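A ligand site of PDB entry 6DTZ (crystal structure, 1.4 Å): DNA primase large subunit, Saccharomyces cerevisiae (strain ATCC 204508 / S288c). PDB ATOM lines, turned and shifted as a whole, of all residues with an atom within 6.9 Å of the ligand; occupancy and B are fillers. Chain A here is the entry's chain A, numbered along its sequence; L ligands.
The side-chain sulfur (SG) of Cys 163 binds an iron atom (FE3) of the ligand (2.3 Å).
FE2 of the ligand is bound by SG of Cys 106, 2.3 Å away.
An iron atom (FE4) of the ligand is bound by the side-chain sulfur (SG) of Cys 123, at 2.3 Å.
The side-chain sulfur (SG) of Cys 25 is bound to an iron atom (FE1) of the ligand.
The backbone NH (N) of Cys 25 sits close to a sulfur (S2) of the ligand (3.4 Å).
SG of Cys 123 lies close to N of Phe 125 (3.7 Å).
O of Thr 160 sits at hydrogen-bond distance from OG1 of Thr 164, 2.8 Å away.
The backbone carbonyl oxygen (O) of Ala 187 lies within hydrogen-bond range of the backbone NH (N) of Cys 106, 3.0 Å away.
The side-chain sulfur (SG) of Cys 106 sits close to the backbone NH (N) of His 188, at 3.4 Å.
Residues that only touch the ligand: Pro 23 (3.7 Å), Ile 109 (3.9 Å), Phe 125 (3.7 Å), Tyr 159 (3.8 Å), Thr 160 (3.9 Å) and Pro 189 (3.6 Å).
Hydrophobic or aromatic side chains that line the ligand: Pro 23, Ile 109, Phe 125 and Pro 189.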
ATOM      1  N   PRO A  23      -0.370   1.942   5.553  1.00  0.00           N
ATOM      2  CA  PRO A  23      -1.788   1.564   5.394  1.00  0.00           C
ATOM      3  C   PRO A  23      -2.381   1.200   6.747  1.00  0.00           C
ATOM      4  O   PRO A  23      -1.685   1.058   7.758  1.00  0.00           O
ATOM      5  CB  PRO A  23      -1.719   0.350   4.465  1.00  0.00           C
ATOM      6  CG  PRO A  23      -0.407  -0.297   4.823  1.00  0.00           C
ATOM      7  CD  PRO A  23       0.553   0.880   5.072  1.00  0.00           C
ATOM      8  N   LEU A  24      -3.725   1.009   6.757  1.00  0.00           N
ATOM      9  CA  LEU A  24      -4.415   0.849   8.027  1.00  0.00           C
ATOM     10  C   LEU A  24      -3.912  -0.345   8.831  1.00  0.00           C
ATOM     11  O   LEU A  24      -3.876  -0.292  10.059  1.00  0.00           O
ATOM     12  CB  LEU A  24      -5.934   0.719   7.824  1.00  0.00           C
ATOM     13  CG  LEU A  24      -6.760   1.960   7.511  1.00  0.00           C
ATOM     14  CD1 LEU A  24      -8.247   1.727   7.838  1.00  0.00           C
ATOM     15  CD2 LEU A  24      -6.194   3.204   8.221  1.00  0.00           C
ATOM     16  N   CYS A  25      -3.574  -1.459   8.158  1.00  0.00           N
ATOM     17  CA  CYS A  25      -3.107  -2.638   8.926  1.00  0.00           C
ATOM     18  C   CYS A  25      -1.840  -2.327   9.704  1.00  0.00           C
ATOM     19  O   CYS A  25      -1.715  -2.707  10.879  1.00  0.00           O
ATOM     20  CB  CYS A  25      -2.884  -3.829   7.991  1.00  0.00           C
ATOM     21  SG  CYS A  25      -1.757  -3.557   6.635  1.00  0.00           S
ATOM     22  N   ILE A  26      -0.894  -1.599   9.079  1.00  0.00           N
ATOM     23  CA  ILE A  26       0.353  -1.266   9.729  1.00  0.00           C
ATOM     24  C   ILE A  26       0.114  -0.231  10.812  1.00  0.00           C
ATOM     25  O   ILE A  26       0.704  -0.303  11.885  1.00  0.00           O
ATOM     26  CB  ILE A  26       1.392  -0.808   8.689  1.00  0.00           C
ATOM     27  CG1 ILE A  26       1.693  -1.918   7.702  1.00  0.00           C
ATOM     28  CG2 ILE A  26       2.667  -0.295   9.399  1.00  0.00           C
ATOM     29  CD1 ILE A  26       2.109  -3.294   8.320  1.00  0.00           C
ATOM     30  N   GLN A  46       3.892  -9.873  10.791  1.00  0.00           N
ATOM     31  CA  GLN A  46       3.384  -8.909   9.810  1.00  0.00           C
ATOM     32  C   GLN A  46       4.110  -7.568   9.899  1.00  0.00           C
ATOM     33  O   GLN A  46       4.563  -7.030   8.872  1.00  0.00           O
ATOM     34  CB  GLN A  46       1.888  -8.691  10.039  1.00  0.00           C
ATOM     35  CG  GLN A  46       1.198  -7.869   8.913  1.00  0.00           C
ATOM     36  CD  GLN A  46      -0.319  -7.856   9.050  1.00  0.00           C
ATOM     37  OE1 GLN A  46      -0.886  -8.742   9.680  1.00  0.00           O
ATOM     38  NE2 GLN A  46      -0.999  -6.866   8.426  1.00  0.00           N
ATOM     39  N   ASP A 105       2.134  -9.793   1.438  1.00  0.00           N
ATOM     40  CA  ASP A 105       1.215  -9.034   0.609  1.00  0.00           C
ATOM     41  C   ASP A 105      -0.203  -9.138   1.183  1.00  0.00           C
ATOM     42  O   ASP A 105      -0.454  -9.828   2.159  1.00  0.00           O
ATOM     43  CB  ASP A 105       1.346  -9.431  -0.856  1.00  0.00           C
ATOM     44  CG  ASP A 105       0.813 -10.806  -1.194  1.00  0.00           C
ATOM     45  OD1 ASP A 105       0.237 -11.497  -0.354  1.00  0.00           O
ATOM     46  OD2 ASP A 105       0.965 -11.211  -2.363  1.00  0.00           O
ATOM     47  N   CYS A 106      -1.150  -8.401   0.571  1.00  0.00           N
ATOM     48  CA  CYS A 106      -2.500  -8.365   1.161  1.00  0.00           C
ATOM     49  C   CYS A 106      -3.172  -9.727   1.116  1.00  0.00           C
ATOM     50  O   CYS A 106      -3.826 -10.100   2.097  1.00  0.00           O
ATOM     51  CB  CYS A 106      -3.406  -7.353   0.450  1.00  0.00           C
ATOM     52  SG  CYS A 106      -2.740  -5.677   0.535  1.00  0.00           S
ATOM     53  N   HIS A 107      -3.020 -10.484   0.032  1.00  0.00           N
ATOM     54  CA  HIS A 107      -3.599 -11.814   0.000  1.00  0.00           C
ATOM     55  C   HIS A 107      -3.050 -12.679   1.112  1.00  0.00           C
ATOM     56  O   HIS A 107      -3.804 -13.422   1.777  1.00  0.00           O
ATOM     57  CB  HIS A 107      -3.340 -12.437  -1.361  1.00  0.00           C
ATOM     58  CG  HIS A 107      -3.982 -13.773  -1.544  1.00  0.00           C
ATOM     59  ND1 HIS A 107      -5.298 -13.928  -1.903  1.00  0.00           N
ATOM     60  CD2 HIS A 107      -3.496 -15.023  -1.362  1.00  0.00           C
ATOM     61  CE1 HIS A 107      -5.598 -15.214  -1.958  1.00  0.00           C
ATOM     62  NE2 HIS A 107      -4.515 -15.900  -1.641  1.00  0.00           N
ATOM     63  N   ILE A 109      -1.747 -11.663   3.980  1.00  0.00           N
ATOM     64  CA  ILE A 109      -2.293 -11.147   5.229  1.00  0.00           C
ATOM     65  C   ILE A 109      -3.722 -11.649   5.447  1.00  0.00           C
ATOM     66  O   ILE A 109      -4.051 -12.159   6.522  1.00  0.00           O
ATOM     67  CB  ILE A 109      -2.212  -9.615   5.253  1.00  0.00           C
ATOM     68  CG1 ILE A 109      -0.771  -9.214   5.480  1.00  0.00           C
ATOM     69  CG2 ILE A 109      -3.080  -9.058   6.364  1.00  0.00           C
ATOM     70  CD1 ILE A 109      -0.543  -7.722   5.090  1.00  0.00           C
ATOM     71  N   LEU A 110      -4.555 -11.509   4.417  1.00  0.00           N
ATOM     72  CA  LEU A 110      -5.951 -11.930   4.528  1.00  0.00           C
ATOM     73  C   LEU A 110      -6.071 -13.425   4.790  1.00  0.00           C
ATOM     74  O   LEU A 110      -7.068 -13.866   5.386  1.00  0.00           O
ATOM     75  CB  LEU A 110      -6.744 -11.489   3.281  1.00  0.00           C
ATOM     76  CG  LEU A 110      -6.995  -9.969   3.231  1.00  0.00           C
ATOM     77  CD1 LEU A 110      -7.342  -9.535   1.819  1.00  0.00           C
ATOM     78  CD2 LEU A 110      -8.103  -9.536   4.217  1.00  0.00           C
ATOM     79  N   GLY A 122      -3.726  -8.781  10.497  1.00  0.00           N
ATOM     80  CA  GLY A 122      -4.887  -8.866   9.643  1.00  0.00           C
ATOM     81  C   GLY A 122      -5.070  -7.604   8.815  1.00  0.00           C
ATOM     82  O   GLY A 122      -4.146  -6.819   8.608  1.00  0.00           O
ATOM     83  N   CYS A 123      -6.308  -7.384   8.388  1.00  0.00           N
ATOM     84  CA  CYS A 123      -6.683  -6.263   7.521  1.00  0.00           C
ATOM     85  C   CYS A 123      -7.858  -5.547   8.184  1.00  0.00           C
ATOM     86  O   CYS A 123      -8.973  -6.102   8.226  1.00  0.00           O
ATOM     87  CB  CYS A 123      -7.083  -6.762   6.135  1.00  0.00           C
ATOM     88  SG  CYS A 123      -7.672  -5.390   5.118  1.00  0.00           S
ATOM     89  N   PRO A 124      -7.674  -4.344   8.707  1.00  0.00           N
ATOM     90  CA  PRO A 124      -8.795  -3.661   9.378  1.00  0.00           C
ATOM     91  C   PRO A 124     -10.045  -3.478   8.520  1.00  0.00           C
ATOM     92  O   PRO A 124     -11.160  -3.408   9.078  1.00  0.00           O
ATOM     93  CB  PRO A 124      -8.210  -2.298   9.771  1.00  0.00           C
ATOM     94  CG  PRO A 124      -6.704  -2.624  10.017  1.00  0.00           C
ATOM     95  CD  PRO A 124      -6.400  -3.647   8.921  1.00  0.00           C
ATOM     96  N   PHE A 125      -9.929  -3.372   7.195  1.00  0.00           N
ATOM     97  CA  PHE A 125     -11.143  -3.219   6.393  1.00  0.00           C
ATOM     98  C   PHE A 125     -12.063  -4.433   6.511  1.00  0.00           C
ATOM     99  O   PHE A 125     -13.278  -4.292   6.326  1.00  0.00           O
ATOM    100  CB  PHE A 125     -10.758  -2.948   4.935  1.00  0.00           C
ATOM    101  CG  PHE A 125     -10.052  -1.642   4.778  1.00  0.00           C
ATOM    102  CD1 PHE A 125     -10.783  -0.426   4.869  1.00  0.00           C
ATOM    103  CD2 PHE A 125      -8.682  -1.595   4.550  1.00  0.00           C
ATOM    104  CE1 PHE A 125     -10.134   0.796   4.764  1.00  0.00           C
ATOM    105  CE2 PHE A 125      -8.037  -0.374   4.454  1.00  0.00           C
ATOM    106  CZ  PHE A 125      -8.737   0.822   4.511  1.00  0.00           C
ATOM    107  N   ARG A 126     -11.505  -5.627   6.799  1.00  0.00           N
ATOM    108  CA  ARG A 126     -12.286  -6.804   7.094  1.00  0.00           C
ATOM    109  C   ARG A 126     -12.541  -6.971   8.580  1.00  0.00           C
ATOM    110  O   ARG A 126     -13.630  -7.382   8.985  1.00  0.00           O
ATOM    111  CB  ARG A 126     -11.542  -8.041   6.575  1.00  0.00           C
ATOM    112  CG  ARG A 126     -12.255  -9.363   6.903  1.00  0.00           C
ATOM    113  CD  ARG A 126     -11.396 -10.563   6.674  1.00  0.00           C
ATOM    114  NE  ARG A 126     -10.278 -10.550   7.609  1.00  0.00           N
ATOM    115  CZ  ARG A 126      -9.196 -11.327   7.537  1.00  0.00           C
ATOM    116  NH1 ARG A 126      -9.133 -12.246   6.556  1.00  0.00           N
ATOM    117  NH2 ARG A 126      -8.228 -11.192   8.432  1.00  0.00           N
ATOM    118  N   TYR A 159     -11.695  -5.779   0.163  1.00  0.00           N
ATOM    119  CA  TYR A 159     -10.883  -5.073   1.154  1.00  0.00           C
ATOM    120  C   TYR A 159      -9.758  -4.274   0.520  1.00  0.00           C
ATOM    121  O   TYR A 159      -9.455  -3.174   0.983  1.00  0.00           O
ATOM    122  CB  TYR A 159     -10.336  -6.034   2.231  1.00  0.00           C
ATOM    123  CG  TYR A 159     -11.440  -6.881   2.779  1.00  0.00           C
ATOM    124  CD1 TYR A 159     -12.546  -6.295   3.400  1.00  0.00           C
ATOM    125  CD2 TYR A 159     -11.430  -8.278   2.627  1.00  0.00           C
ATOM    126  CE1 TYR A 159     -13.603  -7.068   3.858  1.00  0.00           C
ATOM    127  CE2 TYR A 159     -12.475  -9.049   3.113  1.00  0.00           C
ATOM    128  CZ  TYR A 159     -13.556  -8.424   3.728  1.00  0.00           C
ATOM    129  OH  TYR A 159     -14.634  -9.166   4.203  1.00  0.00           O
ATOM    130  N   THR A 160      -9.127  -4.806  -0.539  1.00  0.00           N
ATOM    131  CA  THR A 160      -8.034  -4.065  -1.162  1.00  0.00           C
ATOM    132  C   THR A 160      -8.561  -2.877  -1.967  1.00  0.00           C
ATOM    133  O   THR A 160      -7.845  -1.895  -2.130  1.00  0.00           O
ATOM    134  CB  THR A 160      -7.155  -4.985  -2.008  1.00  0.00           C
ATOM    135  OG1 THR A 160      -7.936  -5.535  -3.075  1.00  0.00           O
ATOM    136  CG2 THR A 160      -6.569  -6.142  -1.162  1.00  0.00           C
ATOM    137  N   ILE A 161      -9.793  -2.970  -2.489  1.00  0.00           N
ATOM    138  CA  ILE A 161     -10.416  -1.797  -3.096  1.00  0.00           C
ATOM    139  C   ILE A 161     -10.718  -0.743  -2.039  1.00  0.00           C
ATOM    140  O   ILE A 161     -10.488   0.450  -2.260  1.00  0.00           O
ATOM    141  CB  ILE A 161     -11.687  -2.182  -3.864  1.00  0.00           C
ATOM    142  CG1 ILE A 161     -11.333  -3.203  -4.970  1.00  0.00           C
ATOM    143  CG2 ILE A 161     -12.362  -0.953  -4.442  1.00  0.00           C
ATOM    144  CD1 ILE A 161     -12.487  -3.424  -6.016  1.00  0.00           C
ATOM    145  N   ALA A 162     -11.244  -1.160  -0.885  1.00  0.00           N
ATOM    146  CA  ALA A 162     -11.471  -0.209   0.192  1.00  0.00           C
ATOM    147  C   ALA A 162     -10.195   0.516   0.555  1.00  0.00           C
ATOM    148  O   ALA A 162     -10.175   1.750   0.709  1.00  0.00           O
ATOM    149  CB  ALA A 162     -12.004  -0.933   1.423  1.00  0.00           C
ATOM    150  N   CYS A 163      -9.093  -0.214   0.631  1.00  0.00           N
ATOM    151  CA  CYS A 163      -7.802   0.362   0.991  1.00  0.00           C
ATOM    152  C   CYS A 163      -7.304   1.295  -0.117  1.00  0.00           C
ATOM    153  O   CYS A 163      -6.751   2.378   0.158  1.00  0.00           O
ATOM    154  CB  CYS A 163      -6.858  -0.820   1.222  1.00  0.00           C
ATOM    155  SG  CYS A 163      -5.165  -0.347   1.837  1.00  0.00           S
ATOM    156  N   THR A 164      -7.524   0.909  -1.373  1.00  0.00           N
ATOM    157  CA  THR A 164      -7.151   1.784  -2.489  1.00  0.00           C
ATOM    158  C   THR A 164      -7.941   3.093  -2.435  1.00  0.00           C
ATOM    159  O   THR A 164      -7.411   4.175  -2.701  1.00  0.00           O
ATOM    160  CB  THR A 164      -7.382   1.061  -3.818  1.00  0.00           C
ATOM    161  OG1 THR A 164      -6.568  -0.135  -3.880  1.00  0.00           O
ATOM    162  CG2 THR A 164      -6.997   1.945  -4.983  1.00  0.00           C
ATOM    163  N   ALA A 187      -1.684  -6.217  -4.831  1.00  0.00           N
ATOM    164  CA  ALA A 187      -2.046  -5.538  -3.587  1.00  0.00           C
ATOM    165  C   ALA A 187      -1.052  -5.864  -2.477  1.00  0.00           C
ATOM    166  O   ALA A 187      -0.840  -7.037  -2.121  1.00  0.00           O
ATOM    167  CB  ALA A 187      -3.436  -5.991  -3.157  1.00  0.00           C
ATOM    168  N   HIS A 188      -0.462  -4.818  -1.881  1.00  0.00           N
ATOM    169  CA  HIS A 188       0.673  -5.030  -0.980  1.00  0.00           C
ATOM    170  C   HIS A 188       0.852  -3.858  -0.033  1.00  0.00           C
ATOM    171  O   HIS A 188       0.939  -2.715  -0.512  1.00  0.00           O
ATOM    172  CB  HIS A 188       1.953  -5.228  -1.812  1.00  0.00           C
ATOM    173  CG  HIS A 188       3.034  -5.954  -1.083  1.00  0.00           C
ATOM    174  ND1 HIS A 188       3.540  -5.530   0.131  1.00  0.00           N
ATOM    175  CD2 HIS A 188       3.751  -7.060  -1.419  1.00  0.00           C
ATOM    176  CE1 HIS A 188       4.489  -6.366   0.532  1.00  0.00           C
ATOM    177  NE2 HIS A 188       4.641  -7.293  -0.399  1.00  0.00           N
ATOM    178  N   PRO A 189       0.856  -4.059   1.289  1.00  0.00           N
ATOM    179  CA  PRO A 189       1.101  -2.930   2.183  1.00  0.00           C
ATOM    180  C   PRO A 189       2.372  -2.164   1.853  1.00  0.00           C
ATOM    181  O   PRO A 189       2.420  -0.930   2.075  1.00  0.00           O
ATOM    182  CB  PRO A 189       1.231  -3.576   3.567  1.00  0.00           C
ATOM    183  CG  PRO A 189       0.517  -4.927   3.416  1.00  0.00           C
ATOM    184  CD  PRO A 189       0.748  -5.360   1.981  1.00  0.00           C
ATOM    185  N   ASN A 190       3.419  -2.852   1.412  1.00  0.00           N
ATOM    186  CA  ASN A 190       4.657  -2.145   1.093  1.00  0.00           C
ATOM    187  C   ASN A 190       4.494  -1.267  -0.131  1.00  0.00           C
ATOM    188  O   ASN A 190       5.177  -0.239  -0.237  1.00  0.00           O
ATOM    189  CB  ASN A 190       5.846  -3.097   0.968  1.00  0.00           C
ATOM    190  CG  ASN A 190       6.277  -3.615   2.307  1.00  0.00           C
ATOM    191  OD1 ASN A 190       5.656  -4.516   2.866  1.00  0.00           O
ATOM    192  ND2 ASN A 190       7.326  -3.006   2.872  1.00  0.00           N
ATOM    193  N   TYR A 192       1.584   0.256  -0.835  1.00  0.00           N
ATOM    194  CA  TYR A 192       0.913   1.433  -0.292  1.00  0.00           C
ATOM    195  C   TYR A 192       1.938   2.386   0.298  1.00  0.00           C
ATOM    196  O   TYR A 192       1.931   3.589   0.006  1.00  0.00           O
ATOM    197  CB  TYR A 192      -0.063   0.975   0.787  1.00  0.00           C
ATOM    198  CG  TYR A 192      -1.067   1.990   1.269  1.00  0.00           C
ATOM    199  CD1 TYR A 192      -0.704   3.109   2.059  1.00  0.00           C
ATOM    200  CD2 TYR A 192      -2.431   1.779   1.013  1.00  0.00           C
ATOM    201  CE1 TYR A 192      -1.659   3.988   2.545  1.00  0.00           C
ATOM    202  CE2 TYR A 192      -3.396   2.646   1.515  1.00  0.00           C
ATOM    203  CZ  TYR A 192      -3.012   3.754   2.247  1.00  0.00           C
ATOM    204  OH  TYR A 192      -3.966   4.605   2.763  1.00  0.00           O
HETATM  205 FE1  LIG L   1      -3.172  -3.682   4.822  1.00  0.00          FE
HETATM  206 FE2  LIG L   1      -3.745  -4.746   2.375  1.00  0.00          FE
HETATM  207 FE3  LIG L   1      -4.660  -2.277   2.996  1.00  0.00          FE
HETATM  208 FE4  LIG L   1      -5.737  -4.462   4.236  1.00  0.00          FE
HETATM  209  S1  LIG L   1      -5.852  -3.969   2.030  1.00  0.00           S
HETATM  210  S2  LIG L   1      -5.066  -2.470   5.239  1.00  0.00           S
HETATM  211  S3  LIG L   1      -3.906  -5.833   4.354  1.00  0.00           S
HETATM  212  S4  LIG L   1      -2.471  -2.864   2.839  1.00  0.00           S
